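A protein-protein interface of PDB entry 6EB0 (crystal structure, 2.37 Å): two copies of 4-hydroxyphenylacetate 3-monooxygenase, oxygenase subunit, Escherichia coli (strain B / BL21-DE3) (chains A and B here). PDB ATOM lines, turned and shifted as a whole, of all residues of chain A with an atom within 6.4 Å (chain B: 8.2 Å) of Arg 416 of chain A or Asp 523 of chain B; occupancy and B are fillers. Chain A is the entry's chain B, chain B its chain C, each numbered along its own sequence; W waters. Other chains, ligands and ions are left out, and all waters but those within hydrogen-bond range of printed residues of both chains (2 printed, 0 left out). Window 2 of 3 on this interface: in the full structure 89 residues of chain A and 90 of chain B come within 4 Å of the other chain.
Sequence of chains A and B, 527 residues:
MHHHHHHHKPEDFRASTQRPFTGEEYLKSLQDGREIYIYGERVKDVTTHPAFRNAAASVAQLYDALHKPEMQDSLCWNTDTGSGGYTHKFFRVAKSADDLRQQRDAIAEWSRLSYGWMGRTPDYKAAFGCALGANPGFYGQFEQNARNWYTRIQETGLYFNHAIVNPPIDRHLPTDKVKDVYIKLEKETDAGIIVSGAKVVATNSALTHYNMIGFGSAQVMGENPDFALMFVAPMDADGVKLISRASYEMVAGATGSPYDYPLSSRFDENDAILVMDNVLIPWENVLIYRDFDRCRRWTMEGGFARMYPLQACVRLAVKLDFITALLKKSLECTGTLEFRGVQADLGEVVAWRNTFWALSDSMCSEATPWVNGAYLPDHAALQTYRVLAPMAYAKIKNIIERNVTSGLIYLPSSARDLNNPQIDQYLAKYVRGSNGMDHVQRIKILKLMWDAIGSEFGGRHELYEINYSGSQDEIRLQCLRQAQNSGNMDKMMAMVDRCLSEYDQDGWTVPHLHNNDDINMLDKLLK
The side-chain amide oxygen of Asn 419 of chain A sits at hydrogen-bond distance from the side-chain amide nitrogen of Gln 505 of chain B.
OD1 of Asp 523 of chain B is in salt-bridge range of NH2 of Arg 416 of chain A, 2.6 Å away.
The backbone NH (N) of Leu 522 of chain B lies within hydrogen-bond range of the side-chain amide oxygen (OD1) of Asn 520 of chain B.
The backbone NH (N) of Arg 416 of chain A lies within hydrogen-bond range of the side-chain hydroxyl (OG) of Ser 414 of chain A (2.9 Å).
ND2 of Asn 419 of chain A is in hydrogen-bond range of O of Ala 415 of chain A (3.4 Å).
OD2 of Asp 260 of chain A is in hydrogen-bond range of OG of Ser 257 of chain A, at 2.7 Å.
OD2 of Asp 260 of chain A sits at hydrogen-bond distance from N of Ala 415 of chain A (3.0 Å).
Among the printed residues, merely in contact across the chains: Arg 416 of chain A with Leu 522 of chain B, Ala 415 of chain A with Gln 505 of chain B, Arg 416 of chain A with Asn 520 of chain B, Asn 419 of chain A with Asp 506 of chain B, Ser 257 of chain A with Asn 516 of chain B and Leu 418 of chain A with Gln 505 of chain B.
Of the printed residues of chain B, Arg 416 of chain A touches Asn 520 (3.7 Å), Leu 522 (3.5 Å) and Asp 523 (2.6 Å).
Asp 523 of chain B touches just one residue of chain A: Arg 416.
Of chain B, only Gln 505 comes within 4 Å of Ala 415 of chain A.
Of the printed residues of chain B, Asn 419 of chain A touches Gln 505 (2.9 Å) and Asp 506 (3.8 Å).
Of the printed residues of chain A, Asn 516 of chain B touches Ser 257.
Of the 12 printed residues of chain A, 5 touch a printed residue of chain B.
Hydrophobic or aromatic side chains of chain A that line the printed part of chain B: Ala 415 and Leu 418.
Of the 11 printed residues of chain B, 6 touch a printed residue of chain A.
Hydrophobic or aromatic side chains of chain B that line the printed part of chain A: Leu 522.
No position is printed for both chains.
Water W2 lies within hydrogen-bond range of the side-chain amide oxygen of Asn 520 of chain B, the guanidinium group of Arg 416 of chain A and the backbone NH of Asp 523 of chain B.
Water W1 lies within hydrogen-bond range of N of Ser 257 of chain A (3.4 Å) and ND2 of Asn 516 of chain B (3.4 Å).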
ATOM      1  N   SER A 257      -6.151 -11.709   4.700  1.00  0.00           N
ATOM      2  CA  SER A 257      -5.075 -12.466   4.087  1.00  0.00           C
ATOM      3  C   SER A 257      -4.704 -11.791   2.775  1.00  0.00           C
ATOM      4  O   SER A 257      -5.423 -10.896   2.320  1.00  0.00           O
ATOM      5  CB  SER A 257      -5.498 -13.911   3.841  1.00  0.00           C
ATOM      6  OG  SER A 257      -6.353 -13.985   2.716  1.00  0.00           O
ATOM      7  N   ASP A 260      -7.472 -12.147   0.420  1.00  0.00           N
ATOM      8  CA  ASP A 260      -8.647 -11.350   0.737  1.00  0.00           C
ATOM      9  C   ASP A 260      -8.411  -9.854   0.547  1.00  0.00           C
ATOM     10  O   ASP A 260      -9.346  -9.133   0.203  1.00  0.00           O
ATOM     11  CB  ASP A 260      -9.094 -11.644   2.167  1.00  0.00           C
ATOM     12  CG  ASP A 260      -9.554 -13.076   2.344  1.00  0.00           C
ATOM     13  OD1 ASP A 260     -10.444 -13.501   1.583  1.00  0.00           O
ATOM     14  OD2 ASP A 260      -9.015 -13.777   3.234  1.00  0.00           O
ATOM     15  N   SER A 413     -16.267 -14.335   3.196  1.00  0.00           N
ATOM     16  CA  SER A 413     -15.438 -13.536   4.101  1.00  0.00           C
ATOM     17  C   SER A 413     -13.948 -13.784   3.924  1.00  0.00           C
ATOM     18  O   SER A 413     -13.148 -12.864   4.101  1.00  0.00           O
ATOM     19  CB  SER A 413     -15.813 -13.816   5.558  1.00  0.00           C
ATOM     20  OG  SER A 413     -15.483 -15.150   5.931  1.00  0.00           O
ATOM     21  N   SER A 414     -13.543 -15.007   3.609  1.00  0.00           N
ATOM     22  CA  SER A 414     -12.167 -15.343   3.920  1.00  0.00           C
ATOM     23  C   SER A 414     -11.660 -16.481   3.054  1.00  0.00           C
ATOM     24  O   SER A 414     -12.408 -17.391   2.687  1.00  0.00           O
ATOM     25  CB  SER A 414     -12.036 -15.725   5.398  1.00  0.00           C
ATOM     26  OG  SER A 414     -10.707 -16.070   5.707  1.00  0.00           O
ATOM     27  N   ALA A 415     -10.357 -16.429   2.765  1.00  0.00           N
ATOM     28  CA  ALA A 415      -9.682 -17.592   2.207  1.00  0.00           C
ATOM     29  C   ALA A 415      -9.906 -18.820   3.086  1.00  0.00           C
ATOM     30  O   ALA A 415      -9.844 -19.950   2.601  1.00  0.00           O
ATOM     31  CB  ALA A 415      -8.186 -17.302   2.045  1.00  0.00           C
ATOM     32  N   ARG A 416     -10.158 -18.610   4.381  1.00  0.00           N
ATOM     33  CA  ARG A 416     -10.527 -19.700   5.276  1.00  0.00           C
ATOM     34  C   ARG A 416     -11.813 -20.388   4.842  1.00  0.00           C
ATOM     35  O   ARG A 416     -11.980 -21.587   5.078  1.00  0.00           O
ATOM     36  CB  ARG A 416     -10.700 -19.178   6.695  1.00  0.00           C
ATOM     37  CG  ARG A 416      -9.461 -18.598   7.292  1.00  0.00           C
ATOM     38  CD  ARG A 416      -9.776 -17.863   8.568  1.00  0.00           C
ATOM     39  NE  ARG A 416      -8.640 -17.955   9.467  1.00  0.00           N
ATOM     40  CZ  ARG A 416      -8.662 -18.618  10.611  1.00  0.00           C
ATOM     41  NH1 ARG A 416      -9.783 -19.204  11.006  1.00  0.00           N
ATOM     42  NH2 ARG A 416      -7.573 -18.669  11.362  1.00  0.00           N
ATOM     43  N   ASP A 417     -12.741 -19.653   4.230  1.00  0.00           N
ATOM     44  CA  ASP A 417     -13.945 -20.308   3.734  1.00  0.00           C
ATOM     45  C   ASP A 417     -13.597 -21.290   2.617  1.00  0.00           C
ATOM     46  O   ASP A 417     -14.141 -22.395   2.565  1.00  0.00           O
ATOM     47  CB  ASP A 417     -14.968 -19.264   3.256  1.00  0.00           C
ATOM     48  CG  ASP A 417     -15.446 -18.330   4.372  1.00  0.00           C
ATOM     49  OD1 ASP A 417     -15.739 -18.824   5.478  1.00  0.00           O
ATOM     50  OD2 ASP A 417     -15.545 -17.093   4.145  1.00  0.00           O
ATOM     51  N   LEU A 418     -12.631 -20.935   1.760  1.00  0.00           N
ATOM     52  CA  LEU A 418     -12.238 -21.818   0.662  1.00  0.00           C
ATOM     53  C   LEU A 418     -11.491 -23.052   1.152  1.00  0.00           C
ATOM     54  O   LEU A 418     -11.567 -24.113   0.526  1.00  0.00           O
ATOM     55  CB  LEU A 418     -11.360 -21.061  -0.335  1.00  0.00           C
ATOM     56  CG  LEU A 418     -11.921 -19.787  -0.968  1.00  0.00           C
ATOM     57  CD1 LEU A 418     -10.844 -19.127  -1.798  1.00  0.00           C
ATOM     58  CD2 LEU A 418     -13.151 -20.068  -1.798  1.00  0.00           C
ATOM     59  N   ASN A 419     -10.753 -22.929   2.246  1.00  0.00           N
ATOM     60  CA  ASN A 419      -9.941 -24.011   2.776  1.00  0.00           C
ATOM     61  C   ASN A 419     -10.707 -24.883   3.757  1.00  0.00           C
ATOM     62  O   ASN A 419     -10.130 -25.797   4.342  1.00  0.00           O
ATOM     63  CB  ASN A 419      -8.688 -23.434   3.437  1.00  0.00           C
ATOM     64  CG  ASN A 419      -7.754 -22.775   2.441  1.00  0.00           C
ATOM     65  OD1 ASN A 419      -7.705 -23.163   1.278  1.00  0.00           O
ATOM     66  ND2 ASN A 419      -7.009 -21.775   2.893  1.00  0.00           N
ATOM     67  N   ASN A 420     -11.991 -24.623   3.945  1.00  0.00           N
ATOM     68  CA  ASN A 420     -12.856 -25.487   4.735  1.00  0.00           C
ATOM     69  C   ASN A 420     -13.815 -26.228   3.800  1.00  0.00           C
ATOM     70  O   ASN A 420     -14.765 -25.626   3.281  1.00  0.00           O
ATOM     71  CB  ASN A 420     -13.618 -24.649   5.761  1.00  0.00           C
ATOM     72  CG  ASN A 420     -14.482 -25.475   6.647  1.00  0.00           C
ATOM     73  OD1 ASN A 420     -14.723 -26.634   6.367  1.00  0.00           O
ATOM     74  ND2 ASN A 420     -14.972 -24.882   7.720  1.00  0.00           N
ATOM     75  N   PRO A 421     -13.592 -27.514   3.514  1.00  0.00           N
ATOM     76  CA  PRO A 421     -14.453 -28.202   2.535  1.00  0.00           C
ATOM     77  C   PRO A 421     -15.922 -28.182   2.903  1.00  0.00           C
ATOM     78  O   PRO A 421     -16.785 -28.175   2.014  1.00  0.00           O
ATOM     79  CB  PRO A 421     -13.889 -29.629   2.511  1.00  0.00           C
ATOM     80  CG  PRO A 421     -13.014 -29.735   3.689  1.00  0.00           C
ATOM     81  CD  PRO A 421     -12.500 -28.373   3.990  1.00  0.00           C
ATOM     82  N   ILE A 423     -17.514 -25.677   3.859  1.00  0.00           N
ATOM     83  CA  ILE A 423     -18.013 -24.456   3.218  1.00  0.00           C
ATOM     84  C   ILE A 423     -17.684 -24.440   1.730  1.00  0.00           C
ATOM     85  O   ILE A 423     -18.530 -24.083   0.913  1.00  0.00           O
ATOM     86  CB  ILE A 423     -17.449 -23.202   3.920  1.00  0.00           C
ATOM     87  CG1 ILE A 423     -17.822 -23.165   5.403  1.00  0.00           C
ATOM     88  CG2 ILE A 423     -17.937 -21.934   3.245  1.00  0.00           C
ATOM     89  CD1 ILE A 423     -16.995 -22.155   6.203  1.00  0.00           C
ATOM     90  N   GLN B 505      -4.726 -18.622  -2.216  1.00  0.00           N
ATOM     91  CA  GLN B 505      -5.506 -18.767  -0.997  1.00  0.00           C
ATOM     92  C   GLN B 505      -4.665 -19.192   0.199  1.00  0.00           C
ATOM     93  O   GLN B 505      -5.180 -19.201   1.317  1.00  0.00           O
ATOM     94  CB  GLN B 505      -6.634 -19.777  -1.242  1.00  0.00           C
ATOM     95  CG  GLN B 505      -6.133 -21.186  -1.594  1.00  0.00           C
ATOM     96  CD  GLN B 505      -7.170 -22.055  -2.310  1.00  0.00           C
ATOM     97  OE1 GLN B 505      -7.166 -22.131  -3.536  1.00  0.00           O
ATOM     98  NE2 GLN B 505      -8.039 -22.731  -1.548  1.00  0.00           N
ATOM     99  N   ASP B 506      -3.381 -19.499   0.001  1.00  0.00           N
ATOM    100  CA  ASP B 506      -2.489 -19.882   1.087  1.00  0.00           C
ATOM    101  C   ASP B 506      -1.465 -18.820   1.451  1.00  0.00           C
ATOM    102  O   ASP B 506      -0.784 -18.967   2.468  1.00  0.00           O
ATOM    103  CB  ASP B 506      -1.751 -21.181   0.734  1.00  0.00           C
ATOM    104  CG  ASP B 506      -2.683 -22.377   0.669  1.00  0.00           C
ATOM    105  OD1 ASP B 506      -3.544 -22.497   1.564  1.00  0.00           O
ATOM    106  OD2 ASP B 506      -2.567 -23.182  -0.278  1.00  0.00           O
ATOM    107  N   ASN B 516       0.948 -13.576   6.732  1.00  0.00           N
ATOM    108  CA  ASN B 516       0.344 -13.048   7.945  1.00  0.00           C
ATOM    109  C   ASN B 516      -0.017 -14.135   8.948  1.00  0.00           C
ATOM    110  O   ASN B 516      -0.751 -13.866   9.904  1.00  0.00           O
ATOM    111  CB  ASN B 516      -0.889 -12.210   7.602  1.00  0.00           C
ATOM    112  CG  ASN B 516      -2.034 -13.045   7.093  1.00  0.00           C
ATOM    113  OD1 ASN B 516      -1.828 -14.044   6.419  1.00  0.00           O
ATOM    114  ND2 ASN B 516      -3.256 -12.648   7.426  1.00  0.00           N
ATOM    115  N   ASP B 517       0.488 -15.354   8.770  1.00  0.00           N
ATOM    116  CA  ASP B 517       0.179 -16.401   9.735  1.00  0.00           C
ATOM    117  C   ASP B 517       0.736 -16.090  11.119  1.00  0.00           C
ATOM    118  O   ASP B 517       0.205 -16.594  12.111  1.00  0.00           O
ATOM    119  CB  ASP B 517       0.665 -17.752   9.215  1.00  0.00           C
ATOM    120  CG  ASP B 517       1.942 -17.639   8.434  1.00  0.00           C
ATOM    121  OD1 ASP B 517       2.804 -16.822   8.822  1.00  0.00           O
ATOM    122  OD2 ASP B 517       2.071 -18.351   7.414  1.00  0.00           O
ATOM    123  N   ASN B 520      -2.164 -13.132  12.116  1.00  0.00           N
ATOM    124  CA  ASN B 520      -3.597 -13.310  11.943  1.00  0.00           C
ATOM    125  C   ASN B 520      -4.237 -13.711  13.269  1.00  0.00           C
ATOM    126  O   ASN B 520      -3.735 -14.588  13.973  1.00  0.00           O
ATOM    127  CB  ASN B 520      -3.891 -14.347  10.857  1.00  0.00           C
ATOM    128  CG  ASN B 520      -5.374 -14.493  10.594  1.00  0.00           C
ATOM    129  OD1 ASN B 520      -6.047 -15.296  11.232  1.00  0.00           O
ATOM    130  ND2 ASN B 520      -5.901 -13.680   9.684  1.00  0.00           N
ATOM    131  N   MET B 521      -5.324 -13.034  13.630  1.00  0.00           N
ATOM    132  CA  MET B 521      -5.968 -13.209  14.922  1.00  0.00           C
ATOM    133  C   MET B 521      -7.278 -13.981  14.842  1.00  0.00           C
ATOM    134  O   MET B 521      -7.991 -14.069  15.844  1.00  0.00           O
ATOM    135  CB  MET B 521      -6.216 -11.845  15.564  1.00  0.00           C
ATOM    136  CG  MET B 521      -4.952 -11.081  15.869  1.00  0.00           C
ATOM    137  SD  MET B 521      -3.945 -11.905  17.108  1.00  0.00           S
ATOM    138  CE  MET B 521      -2.382 -11.071  16.900  1.00  0.00           C
ATOM    139  N   LEU B 522      -7.628 -14.531  13.682  1.00  0.00           N
ATOM    140  CA  LEU B 522      -8.945 -15.142  13.542  1.00  0.00           C
ATOM    141  C   LEU B 522      -9.090 -16.377  14.431  1.00  0.00           C
ATOM    142  O   LEU B 522     -10.135 -16.574  15.060  1.00  0.00           O
ATOM    143  CB  LEU B 522      -9.221 -15.462  12.075  1.00  0.00           C
ATOM    144  CG  LEU B 522      -9.326 -14.203  11.194  1.00  0.00           C
ATOM    145  CD1 LEU B 522      -9.384 -14.527   9.711  1.00  0.00           C
ATOM    146  CD2 LEU B 522     -10.509 -13.346  11.594  1.00  0.00           C
ATOM    147  N   ASP B 523      -8.054 -17.209  14.519  1.00  0.00           N
ATOM    148  CA  ASP B 523      -8.112 -18.348  15.430  1.00  0.00           C
ATOM    149  C   ASP B 523      -8.406 -17.900  16.851  1.00  0.00           C
ATOM    150  O   ASP B 523      -9.297 -18.441  17.512  1.00  0.00           O
ATOM    151  CB  ASP B 523      -6.808 -19.134  15.377  1.00  0.00           C
ATOM    152  CG  ASP B 523      -6.725 -20.013  14.169  1.00  0.00           C
ATOM    153  OD1 ASP B 523      -7.747 -20.134  13.473  1.00  0.00           O
ATOM    154  OD2 ASP B 523      -5.647 -20.570  13.897  1.00  0.00           O
ATOM    155  N   LYS B 524      -7.660 -16.914  17.344  1.00  0.00           N
ATOM    156  CA  LYS B 524      -7.904 -16.419  18.692  1.00  0.00           C
ATOM    157  C   LYS B 524      -9.309 -15.845  18.821  1.00  0.00           C
ATOM    158  O   LYS B 524      -9.988 -16.066  19.828  1.00  0.00           O
ATOM    159  CB  LYS B 524      -6.848 -15.377  19.070  1.00  0.00           C
ATOM    160  CG  LYS B 524      -5.556 -15.980  19.621  1.00  0.00           C
ATOM    161  CD  LYS B 524      -4.581 -14.911  20.107  1.00  0.00           C
ATOM    162  CE  LYS B 524      -3.585 -15.471  21.125  1.00  0.00           C
ATOM    163  NZ  LYS B 524      -2.698 -16.516  20.549  1.00  0.00           N
ATOM    164  N   LEU B 525      -9.772 -15.117  17.807  1.00  0.00           N
ATOM    165  CA  LEU B 525     -11.088 -14.503  17.903  1.00  0.00           C
ATOM    166  C   LEU B 525     -12.206 -15.528  17.792  1.00  0.00           C
ATOM    167  O   LEU B 525     -13.242 -15.372  18.444  1.00  0.00           O
ATOM    168  CB  LEU B 525     -11.253 -13.421  16.829  1.00  0.00           C
ATOM    169  CG  LEU B 525     -10.581 -12.069  17.075  1.00  0.00           C
ATOM    170  CD1 LEU B 525     -10.426 -11.297  15.780  1.00  0.00           C
ATOM    171  CD2 LEU B 525     -11.394 -11.268  18.064  1.00  0.00           C
ATOM    172  N   LEU B 526     -12.023 -16.576  16.993  1.00  0.00           N
ATOM    173  CA  LEU B 526     -13.109 -17.520  16.728  1.00  0.00           C
ATOM    174  C   LEU B 526     -12.780 -18.927  17.202  1.00  0.00           C
ATOM    175  O   LEU B 526     -13.372 -19.409  18.160  1.00  0.00           O
ATOM    176  CB  LEU B 526     -13.442 -17.552  15.240  1.00  0.00           C
ATOM    177  CG  LEU B 526     -13.551 -16.183  14.581  1.00  0.00           C
ATOM    178  CD1 LEU B 526     -13.847 -16.310  13.092  1.00  0.00           C
ATOM    179  CD2 LEU B 526     -14.608 -15.362  15.284  1.00  0.00           C
HETATM  180  O   HOH W   1      -3.203 -10.139   5.067  1.00  0.00           O
HETATM  181  O   HOH W   2      -5.328 -17.444  12.506  1.00  0.00           O
